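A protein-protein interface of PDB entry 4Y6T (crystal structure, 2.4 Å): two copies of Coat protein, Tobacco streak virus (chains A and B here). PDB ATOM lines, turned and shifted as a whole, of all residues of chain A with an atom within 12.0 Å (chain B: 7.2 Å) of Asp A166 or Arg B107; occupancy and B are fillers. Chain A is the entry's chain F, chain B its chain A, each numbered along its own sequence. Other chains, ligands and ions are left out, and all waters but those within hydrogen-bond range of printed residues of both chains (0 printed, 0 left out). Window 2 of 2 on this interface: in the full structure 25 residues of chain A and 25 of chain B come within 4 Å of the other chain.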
ATOM      1  N   PRO A 158       6.237 -16.720  31.308  1.00  0.00           N
ATOM      2  CA  PRO A 158       6.286 -15.533  32.180  1.00  0.00           C
ATOM      3  C   PRO A 158       4.923 -14.910  32.394  1.00  0.00           C
ATOM      4  O   PRO A 158       4.100 -14.862  31.483  1.00  0.00           O
ATOM      5  CB  PRO A 158       7.192 -14.559  31.416  1.00  0.00           C
ATOM      6  CG  PRO A 158       7.957 -15.393  30.463  1.00  0.00           C
ATOM      7  CD  PRO A 158       7.089 -16.577  30.128  1.00  0.00           C
ATOM      8  N   ASP A 160       3.751 -11.970  32.561  1.00  0.00           N
ATOM      9  CA  ASP A 160       3.333 -10.851  31.765  1.00  0.00           C
ATOM     10  C   ASP A 160       3.589 -11.090  30.252  1.00  0.00           C
ATOM     11  O   ASP A 160       3.776 -10.126  29.487  1.00  0.00           O
ATOM     12  CB  ASP A 160       3.976  -9.599  32.337  1.00  0.00           C
ATOM     13  CG  ASP A 160       3.305  -9.156  33.700  1.00  0.00           C
ATOM     14  OD1 ASP A 160       2.074  -9.268  33.865  1.00  0.00           O
ATOM     15  OD2 ASP A 160       4.031  -8.721  34.633  1.00  0.00           O
ATOM     16  N   PHE A 161       3.629 -12.353  29.824  1.00  0.00           N
ATOM     17  CA  PHE A 161       3.938 -12.641  28.426  1.00  0.00           C
ATOM     18  C   PHE A 161       2.899 -12.083  27.496  1.00  0.00           C
ATOM     19  O   PHE A 161       3.226 -11.638  26.394  1.00  0.00           O
ATOM     20  CB  PHE A 161       4.059 -14.119  28.182  1.00  0.00           C
ATOM     21  CG  PHE A 161       4.658 -14.475  26.896  1.00  0.00           C
ATOM     22  CD1 PHE A 161       3.894 -14.623  25.779  1.00  0.00           C
ATOM     23  CD2 PHE A 161       6.021 -14.688  26.797  1.00  0.00           C
ATOM     24  CE1 PHE A 161       4.466 -14.967  24.594  1.00  0.00           C
ATOM     25  CE2 PHE A 161       6.594 -15.074  25.601  1.00  0.00           C
ATOM     26  CZ  PHE A 161       5.808 -15.192  24.493  1.00  0.00           C
ATOM     27  N   LEU A 162       1.646 -12.093  27.912  1.00  0.00           N
ATOM     28  CA  LEU A 162       0.562 -11.615  27.058  1.00  0.00           C
ATOM     29  C   LEU A 162       0.151 -10.186  27.231  1.00  0.00           C
ATOM     30  O   LEU A 162      -0.985  -9.811  26.928  1.00  0.00           O
ATOM     31  CB  LEU A 162      -0.617 -12.520  27.228  1.00  0.00           C
ATOM     32  CG  LEU A 162      -0.375 -13.908  26.637  1.00  0.00           C
ATOM     33  CD1 LEU A 162      -1.600 -14.796  26.928  1.00  0.00           C
ATOM     34  CD2 LEU A 162      -0.163 -13.830  25.135  1.00  0.00           C
ATOM     35  N   VAL A 163       1.025  -9.328  27.709  1.00  0.00           N
ATOM     36  CA  VAL A 163       0.792  -7.893  27.538  1.00  0.00           C
ATOM     37  C   VAL A 163       0.625  -7.488  26.049  1.00  0.00           C
ATOM     38  O   VAL A 163       1.280  -8.044  25.153  1.00  0.00           O
ATOM     39  CB  VAL A 163       1.961  -7.132  28.184  1.00  0.00           C
ATOM     40  CG1 VAL A 163       2.019  -5.691  27.709  1.00  0.00           C
ATOM     41  CG2 VAL A 163       1.790  -7.174  29.716  1.00  0.00           C
ATOM     42  N   ASN A 164      -0.327  -6.607  25.787  1.00  0.00           N
ATOM     43  CA  ASN A 164      -0.639  -6.117  24.435  1.00  0.00           C
ATOM     44  C   ASN A 164      -0.877  -7.240  23.440  1.00  0.00           C
ATOM     45  O   ASN A 164      -0.191  -7.368  22.423  1.00  0.00           O
ATOM     46  CB  ASN A 164       0.478  -5.169  23.977  1.00  0.00           C
ATOM     47  CG  ASN A 164       0.128  -4.436  22.703  1.00  0.00           C
ATOM     48  OD1 ASN A 164      -1.034  -4.156  22.422  1.00  0.00           O
ATOM     49  ND2 ASN A 164       1.151  -4.086  21.928  1.00  0.00           N
ATOM     50  N   GLN A 165      -1.856  -8.080  23.778  1.00  0.00           N
ATOM     51  CA  GLN A 165      -2.247  -9.230  22.966  1.00  0.00           C
ATOM     52  C   GLN A 165      -3.512  -8.967  22.167  1.00  0.00           C
ATOM     53  O   GLN A 165      -3.877  -9.836  21.356  1.00  0.00           O
ATOM     54  CB  GLN A 165      -2.439 -10.478  23.878  1.00  0.00           C
ATOM     55  CG  GLN A 165      -3.711 -10.404  24.727  1.00  0.00           C
ATOM     56  CD  GLN A 165      -4.035 -11.652  25.518  1.00  0.00           C
ATOM     57  OE1 GLN A 165      -4.071 -11.584  26.747  1.00  0.00           O
ATOM     58  NE2 GLN A 165      -4.226 -12.797  24.843  1.00  0.00           N
ATOM     59  N   ASP A 166      -4.106  -7.801  22.405  1.00  0.00           N
ATOM     60  CA  ASP A 166      -5.531  -7.320  22.125  1.00  0.00           C
ATOM     61  C   ASP A 166      -6.641  -7.550  23.216  1.00  0.00           C
ATOM     62  O   ASP A 166      -6.917  -6.709  24.110  1.00  0.00           O
ATOM     63  CB  ASP A 166      -6.080  -7.845  20.836  1.00  0.00           C
ATOM     64  CG  ASP A 166      -5.277  -7.378  19.683  1.00  0.00           C
ATOM     65  OD1 ASP A 166      -4.860  -6.199  19.699  1.00  0.00           O
ATOM     66  OD2 ASP A 166      -5.026  -8.189  18.783  1.00  0.00           O
ATOM     67  N   ILE B  69       3.005 -16.023  21.065  1.00  0.00           N
ATOM     68  CA  ILE B  69       4.204 -15.354  20.618  1.00  0.00           C
ATOM     69  C   ILE B  69       4.254 -13.991  21.192  1.00  0.00           C
ATOM     70  O   ILE B  69       3.210 -13.357  21.501  1.00  0.00           O
ATOM     71  CB  ILE B  69       4.333 -15.298  19.112  1.00  0.00           C
ATOM     72  CG1 ILE B  69       3.355 -14.347  18.517  1.00  0.00           C
ATOM     73  CG2 ILE B  69       4.115 -16.671  18.422  1.00  0.00           C
ATOM     74  CD1 ILE B  69       3.697 -14.009  17.072  1.00  0.00           C
ATOM     75  N   GLY B  70       5.483 -13.532  21.356  1.00  0.00           N
ATOM     76  CA  GLY B  70       5.726 -12.155  21.762  1.00  0.00           C
ATOM     77  C   GLY B  70       6.907 -11.591  20.998  1.00  0.00           C
ATOM     78  O   GLY B  70       7.871 -12.351  20.672  1.00  0.00           O
ATOM     79  N   PHE B  71       6.805 -10.325  20.589  1.00  0.00           N
ATOM     80  CA  PHE B  71       7.863  -9.752  19.777  1.00  0.00           C
ATOM     81  C   PHE B  71       7.903  -8.253  19.862  1.00  0.00           C
ATOM     82  O   PHE B  71       6.983  -7.586  20.329  1.00  0.00           O
ATOM     83  CB  PHE B  71       7.758 -10.176  18.338  1.00  0.00           C
ATOM     84  CG  PHE B  71       6.535  -9.684  17.654  1.00  0.00           C
ATOM     85  CD1 PHE B  71       6.521  -8.461  17.003  1.00  0.00           C
ATOM     86  CD2 PHE B  71       5.420 -10.456  17.610  1.00  0.00           C
ATOM     87  CE1 PHE B  71       5.376  -8.028  16.318  1.00  0.00           C
ATOM     88  CE2 PHE B  71       4.274 -10.016  17.000  1.00  0.00           C
ATOM     89  CZ  PHE B  71       4.240  -8.811  16.335  1.00  0.00           C
ATOM     90  N   VAL B  72       9.043  -7.733  19.424  1.00  0.00           N
ATOM     91  CA  VAL B  72       9.236  -6.316  19.241  1.00  0.00           C
ATOM     92  C   VAL B  72       9.790  -6.144  17.824  1.00  0.00           C
ATOM     93  O   VAL B  72      10.711  -6.845  17.450  1.00  0.00           O
ATOM     94  CB  VAL B  72      10.249  -5.797  20.250  1.00  0.00           C
ATOM     95  CG1 VAL B  72      10.650  -4.376  19.917  1.00  0.00           C
ATOM     96  CG2 VAL B  72       9.630  -5.765  21.605  1.00  0.00           C
ATOM     97  N   ALA B  73       9.241  -5.201  17.074  1.00  0.00           N
ATOM     98  CA  ALA B  73       9.642  -4.959  15.717  1.00  0.00           C
ATOM     99  C   ALA B  73      10.173  -3.516  15.560  1.00  0.00           C
ATOM    100  O   ALA B  73       9.862  -2.634  16.340  1.00  0.00           O
ATOM    101  CB  ALA B  73       8.495  -5.174  14.793  1.00  0.00           C
ATOM    102  N   PHE B  79       0.664  -8.561  11.094  1.00  0.00           N
ATOM    103  CA  PHE B  79       0.971  -9.978  11.113  1.00  0.00           C
ATOM    104  C   PHE B  79      -0.252 -10.793  11.329  1.00  0.00           C
ATOM    105  O   PHE B  79      -1.347 -10.265  11.533  1.00  0.00           O
ATOM    106  CB  PHE B  79       1.986 -10.274  12.203  1.00  0.00           C
ATOM    107  CG  PHE B  79       1.460 -10.214  13.606  1.00  0.00           C
ATOM    108  CD1 PHE B  79       0.962  -9.068  14.142  1.00  0.00           C
ATOM    109  CD2 PHE B  79       1.433 -11.355  14.370  1.00  0.00           C
ATOM    110  CE1 PHE B  79       0.474  -9.031  15.447  1.00  0.00           C
ATOM    111  CE2 PHE B  79       0.911 -11.357  15.665  1.00  0.00           C
ATOM    112  CZ  PHE B  79       0.437 -10.192  16.220  1.00  0.00           C
ATOM    113  N   ARG B  98      -6.251 -10.017  10.283  1.00  0.00           N
ATOM    114  CA  ARG B  98      -5.008  -9.192  10.226  1.00  0.00           C
ATOM    115  C   ARG B  98      -4.767  -8.256  11.412  1.00  0.00           C
ATOM    116  O   ARG B  98      -5.586  -7.379  11.673  1.00  0.00           O
ATOM    117  CB  ARG B  98      -4.979  -8.346   8.948  1.00  0.00           C
ATOM    118  CG  ARG B  98      -3.910  -7.277   8.821  1.00  0.00           C
ATOM    119  CD  ARG B  98      -3.652  -6.942   7.357  1.00  0.00           C
ATOM    120  N   LEU B  99      -3.628  -8.423  12.092  1.00  0.00           N
ATOM    121  CA  LEU B  99      -3.338  -7.721  13.333  1.00  0.00           C
ATOM    122  C   LEU B  99      -2.259  -6.720  13.115  1.00  0.00           C
ATOM    123  O   LEU B  99      -1.358  -6.950  12.316  1.00  0.00           O
ATOM    124  CB  LEU B  99      -2.894  -8.700  14.383  1.00  0.00           C
ATOM    125  CG  LEU B  99      -3.934  -9.832  14.576  1.00  0.00           C
ATOM    126  CD1 LEU B  99      -3.301 -11.098  15.110  1.00  0.00           C
ATOM    127  CD2 LEU B  99      -4.991  -9.294  15.534  1.00  0.00           C
ATOM    128  N   GLY B 100      -2.337  -5.610  13.828  1.00  0.00           N
ATOM    129  CA  GLY B 100      -1.376  -4.539  13.677  1.00  0.00           C
ATOM    130  C   GLY B 100      -0.330  -4.542  14.788  1.00  0.00           C
ATOM    131  O   GLY B 100      -0.557  -5.070  15.870  1.00  0.00           O
ATOM    132  N   PHE B 101       0.854  -3.990  14.502  1.00  0.00           N
ATOM    133  CA  PHE B 101       1.806  -3.692  15.565  1.00  0.00           C
ATOM    134  C   PHE B 101       2.510  -2.403  15.279  1.00  0.00           C
ATOM    135  O   PHE B 101       2.568  -1.942  14.135  1.00  0.00           O
ATOM    136  CB  PHE B 101       2.791  -4.842  15.774  1.00  0.00           C
ATOM    137  CG  PHE B 101       3.564  -5.209  14.561  1.00  0.00           C
ATOM    138  CD1 PHE B 101       4.684  -4.521  14.200  1.00  0.00           C
ATOM    139  CD2 PHE B 101       3.155  -6.247  13.772  1.00  0.00           C
ATOM    140  CE1 PHE B 101       5.397  -4.893  13.088  1.00  0.00           C
ATOM    141  CE2 PHE B 101       3.868  -6.624  12.635  1.00  0.00           C
ATOM    142  CZ  PHE B 101       4.993  -5.940  12.295  1.00  0.00           C
ATOM    143  N   LYS B 102       3.044  -1.822  16.332  1.00  0.00           N
ATOM    144  CA  LYS B 102       3.710  -0.560  16.281  1.00  0.00           C
ATOM    145  C   LYS B 102       5.187  -0.790  16.529  1.00  0.00           C
ATOM    146  O   LYS B 102       5.590  -1.650  17.304  1.00  0.00           O
ATOM    147  CB  LYS B 102       3.206   0.376  17.383  1.00  0.00           C
ATOM    148  CG  LYS B 102       1.743   0.674  17.314  1.00  0.00           C
ATOM    149  CD  LYS B 102       1.504   1.743  16.262  1.00  0.00           C
ATOM    150  CE  LYS B 102       0.004   1.970  15.993  1.00  0.00           C
ATOM    151  NZ  LYS B 102      -0.290   2.667  14.688  1.00  0.00           N
ATOM    152  N   ASN B 104       8.719  -0.648  18.011  1.00  0.00           N
ATOM    153  CA  ASN B 104       9.344  -0.589  19.318  1.00  0.00           C
ATOM    154  C   ASN B 104       8.370  -0.817  20.447  1.00  0.00           C
ATOM    155  O   ASN B 104       8.517  -0.272  21.511  1.00  0.00           O
ATOM    156  CB  ASN B 104      10.050   0.738  19.490  1.00  0.00           C
ATOM    157  CG  ASN B 104      11.228   0.930  18.514  1.00  0.00           C
ATOM    158  OD1 ASN B 104      11.830  -0.018  18.050  1.00  0.00           O
ATOM    159  ND2 ASN B 104      11.578   2.164  18.265  1.00  0.00           N
ATOM    160  N   THR B 105       7.352  -1.613  20.188  1.00  0.00           N
ATOM    161  CA  THR B 105       6.325  -1.818  21.152  1.00  0.00           C
ATOM    162  C   THR B 105       6.079  -3.299  21.272  1.00  0.00           C
ATOM    163  O   THR B 105       5.625  -3.945  20.308  1.00  0.00           O
ATOM    164  CB  THR B 105       5.082  -1.085  20.698  1.00  0.00           C
ATOM    165  OG1 THR B 105       5.444   0.254  20.447  1.00  0.00           O
ATOM    166  CG2 THR B 105       3.963  -1.096  21.762  1.00  0.00           C
ATOM    167  N   TYR B 106       6.338  -3.855  22.449  1.00  0.00           N
ATOM    168  CA  TYR B 106       6.081  -5.298  22.673  1.00  0.00           C
ATOM    169  C   TYR B 106       4.654  -5.653  22.257  1.00  0.00           C
ATOM    170  O   TYR B 106       3.683  -4.937  22.592  1.00  0.00           O
ATOM    171  CB  TYR B 106       6.281  -5.673  24.178  1.00  0.00           C
ATOM    172  CG  TYR B 106       6.103  -7.182  24.452  1.00  0.00           C
ATOM    173  CD1 TYR B 106       7.106  -8.095  24.189  1.00  0.00           C
ATOM    174  CD2 TYR B 106       4.875  -7.684  24.920  1.00  0.00           C
ATOM    175  CE1 TYR B 106       6.932  -9.458  24.409  1.00  0.00           C
ATOM    176  CE2 TYR B 106       4.716  -9.034  25.187  1.00  0.00           C
ATOM    177  CZ  TYR B 106       5.721  -9.904  24.936  1.00  0.00           C
ATOM    178  OH  TYR B 106       5.542 -11.257  25.156  1.00  0.00           O
ATOM    179  N   ARG B 107       4.542  -6.712  21.498  1.00  0.00           N
ATOM    180  CA  ARG B 107       3.261  -7.177  20.955  1.00  0.00           C
ATOM    181  C   ARG B 107       3.223  -8.655  21.184  1.00  0.00           C
ATOM    182  O   ARG B 107       4.251  -9.349  20.967  1.00  0.00           O
ATOM    183  CB  ARG B 107       3.228  -7.025  19.462  1.00  0.00           C
ATOM    184  CG  ARG B 107       1.892  -7.306  18.817  1.00  0.00           C
ATOM    185  CD  ARG B 107       0.886  -6.314  19.250  1.00  0.00           C
ATOM    186  NE  ARG B 107      -0.256  -6.294  18.338  1.00  0.00           N
ATOM    187  CZ  ARG B 107      -1.434  -6.860  18.579  1.00  0.00           C
ATOM    188  NH1 ARG B 107      -1.637  -7.523  19.710  1.00  0.00           N
ATOM    189  NH2 ARG B 107      -2.423  -6.757  17.679  1.00  0.00           N
ATOM    190  N   SER B 108       2.051  -9.172  21.586  1.00  0.00           N
ATOM    191  CA  SER B 108       1.874 -10.617  21.777  1.00  0.00           C
ATOM    192  C   SER B 108       0.614 -11.044  21.163  1.00  0.00           C
ATOM    193  O   SER B 108      -0.178 -10.246  20.737  1.00  0.00           O
ATOM    194  CB  SER B 108       1.854 -11.003  23.251  1.00  0.00           C
ATOM    195  OG  SER B 108       0.792 -10.309  23.938  1.00  0.00           O
ATOM    196  N   ARG B 109       0.459 -12.361  21.041  1.00  0.00           N
ATOM    197  CA  ARG B 109      -0.750 -12.895  20.522  1.00  0.00           C
ATOM    198  C   ARG B 109      -0.862 -14.297  21.037  1.00  0.00           C
ATOM    199  O   ARG B 109       0.123 -15.032  21.116  1.00  0.00           O
ATOM    200  CB  ARG B 109      -0.731 -12.890  18.983  1.00  0.00           C
ATOM    201  CG  ARG B 109      -2.023 -13.294  18.311  1.00  0.00           C
ATOM    202  CD  ARG B 109      -3.161 -12.370  18.688  1.00  0.00           C
ATOM    203  NE  ARG B 109      -4.386 -12.637  17.917  1.00  0.00           N
ATOM    204  CZ  ARG B 109      -5.484 -11.917  18.021  1.00  0.00           C
ATOM    205  NH1 ARG B 109      -5.536 -10.846  18.820  1.00  0.00           N
ATOM    206  NH2 ARG B 109      -6.560 -12.276  17.331  1.00  0.00           N
ATOM    207  N   TRP B 128       4.684 -11.850   8.910  1.00  0.00           N
ATOM    208  CA  TRP B 128       4.830 -10.435   9.268  1.00  0.00           C
ATOM    209  C   TRP B 128       5.045  -9.600   7.981  1.00  0.00           C
ATOM    210  O   TRP B 128       5.698 -10.051   7.072  1.00  0.00           O
ATOM    211  CB  TRP B 128       6.055 -10.270  10.112  1.00  0.00           C
ATOM    212  CG  TRP B 128       5.930 -10.673  11.507  1.00  0.00           C
ATOM    213  CD1 TRP B 128       5.702  -9.832  12.609  1.00  0.00           C
ATOM    214  CD2 TRP B 128       6.116 -11.969  12.024  1.00  0.00           C
ATOM    215  NE1 TRP B 128       5.734 -10.545  13.754  1.00  0.00           N
ATOM    216  CE2 TRP B 128       5.983 -11.863  13.432  1.00  0.00           C
ATOM    217  CE3 TRP B 128       6.368 -13.202  11.456  1.00  0.00           C
ATOM    218  CZ2 TRP B 128       6.067 -12.977  14.260  1.00  0.00           C
ATOM    219  CZ3 TRP B 128       6.496 -14.289  12.249  1.00  0.00           C
ATOM    220  CH2 TRP B 128       6.308 -14.197  13.653  1.00  0.00           C
ATOM    221  N   GLN B 141      12.220  -9.194  16.600  1.00  0.00           N
ATOM    222  CA  GLN B 141      12.858  -9.983  17.618  1.00  0.00           C
ATOM    223  C   GLN B 141      11.774 -10.702  18.439  1.00  0.00           C
ATOM    224  O   GLN B 141      10.992 -10.064  19.165  1.00  0.00           O
ATOM    225  CB  GLN B 141      13.642  -9.072  18.560  1.00  0.00           C
ATOM    226  CG  GLN B 141      14.700  -8.243  17.840  1.00  0.00           C
ATOM    227  CD  GLN B 141      15.334  -7.144  18.736  1.00  0.00           C
ATOM    228  OE1 GLN B 141      16.005  -7.412  19.748  1.00  0.00           O
ATOM    229  NE2 GLN B 141      15.115  -5.914  18.358  1.00  0.00           N
ATOM    230  N   LEU B 142      11.782 -12.016  18.352  1.00  0.00           N
ATOM    231  CA  LEU B 142      10.839 -12.857  19.019  1.00  0.00           C
ATOM    232  C   LEU B 142      11.365 -13.335  20.344  1.00  0.00           C
ATOM    233  O   LEU B 142      12.485 -13.791  20.447  1.00  0.00           O
ATOM    234  CB  LEU B 142      10.565 -14.095  18.201  1.00  0.00           C
ATOM    235  CG  LEU B 142       9.600 -13.754  17.080  1.00  0.00           C
ATOM    236  CD1 LEU B 142       9.890 -14.598  15.847  1.00  0.00           C
ATOM    237  CD2 LEU B 142       8.156 -14.004  17.567  1.00  0.00           C
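The side-chain hydroxyl (OH) of Tyr B106 sits at hydrogen-bond distance from the backbone carbonyl oxygen (O) of Phe A161 (2.7 Å). The side-chain amide nitrogen (ND2) of Asn A164 lies within hydrogen-bond range of the backbone carbonyl oxygen (O) of Tyr B106 (2.8 Å). The guanidinium group (NH1) of Arg B107 is in hydrogen-bond range of the backbone carbonyl oxygen (O) of Asn A164, at 3.1 Å. The side-chain carboxylate of Asp A166 is in salt-bridge range of the guanidinium group of Arg B107 (3.2 Å). The backbone carbonyl oxygen (O) of Val A163 is in hydrogen-bond range of the side-chain hydroxyl (OG) of Ser B108, 2.6 Å away. The backbone NH (N) of Ser B108 is in hydrogen-bond range of the backbone carbonyl oxygen (O) of Asn A164 (3.0 Å). The backbone NH (N) of Gln A165 sits close to the side-chain hydroxyl (OG) of Ser B108, 3.5 Å away. O of Gln A165 is in hydrogen-bond range of NH1 of Arg B109. NH1 of Arg B109 is in salt-bridge range of OD2 of Asp A166 (2.7 Å).
The backbone carbonyl oxygen (O) of Ile B69 sits at hydrogen-bond distance from the backbone NH (N) of Arg B109, 3.0 Å away. The backbone NH (N) of Phe B71 sits at hydrogen-bond distance from the backbone carbonyl oxygen (O) of Arg B107. The backbone carbonyl oxygen (O) of Leu B99 sits at hydrogen-bond distance from the backbone NH (N) of Phe B79 (2.9 Å). The guanidinium group of Arg B107 lies within hydrogen-bond range of the backbone carbonyl oxygen of Gly B100.
Phe A161 touches Ile B69. CZ of Phe A161 touches N of Gly B70, 3.6 Å away. Phe A161 touches Ser B108 (O to CB, 3.5 Å). Leu A162 touches Ser B108. Val A163 touches Tyr B106 (O to CE2, 3.6 Å). Gln A165 touches Arg B107. Leu B99 touches Asp A166 (CD2 to OD2, 3.4 Å).
Asp A166 touches just these residues of chain B: Leu B99, Arg B107 and Arg B109. Arg B107 touches three residues of chain A. Of chain A, only Phe A161 comes within 4 Å of Ile B69. Gly B70 touches just one residue of chain A: Phe A161. No residue of chain A comes within 4 Å of Phe B71. Leu B99 touches one residue of chain A. No residue of chain A comes within 4 Å of Phe B101. No residue of chain A comes within 4 Å of Thr B105. Printed residues of chain A within 4 Å of Ser B108: Phe A161, Leu A162, Val A163, Asn A164 and Gln A165. Of chain A, only Gln A165 (3.2 Å) and Asp A166 (2.7 Å) come within 4 Å of Arg B109. Of the printed residues of chain B, Leu A162 touches Ser B108 (3.4 Å). Printed residues of chain B within 4 Å of Asn A164: Tyr B106, Arg B107 and Ser B108. Of the printed residues of chain B, Phe A161 touches Ile B69 (3.5 Å), Gly B70 (3.6 Å), Tyr B106 (2.7 Å) and Ser B108 (3.5 Å). Asn B104 touches none of the printed residues of chain A. Lys B102 touches none of the printed residues of chain A. The nearest residue of chain B that does not touch Asp A166 is Ser B108 (4.9 Å). The nearest printed residue of chain B that does not touch Gln A165 is Leu B99 (6.0 Å).
Printed residues of chain B that touch a printed residue of chain A: Ile B69, Gly B70, Leu B99, Tyr B106, Arg B107, Ser B108 and Arg B109. Along chain B the printed residues that touch a printed residue of chain A span positions 69 to 109.
No position is printed for both chains.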
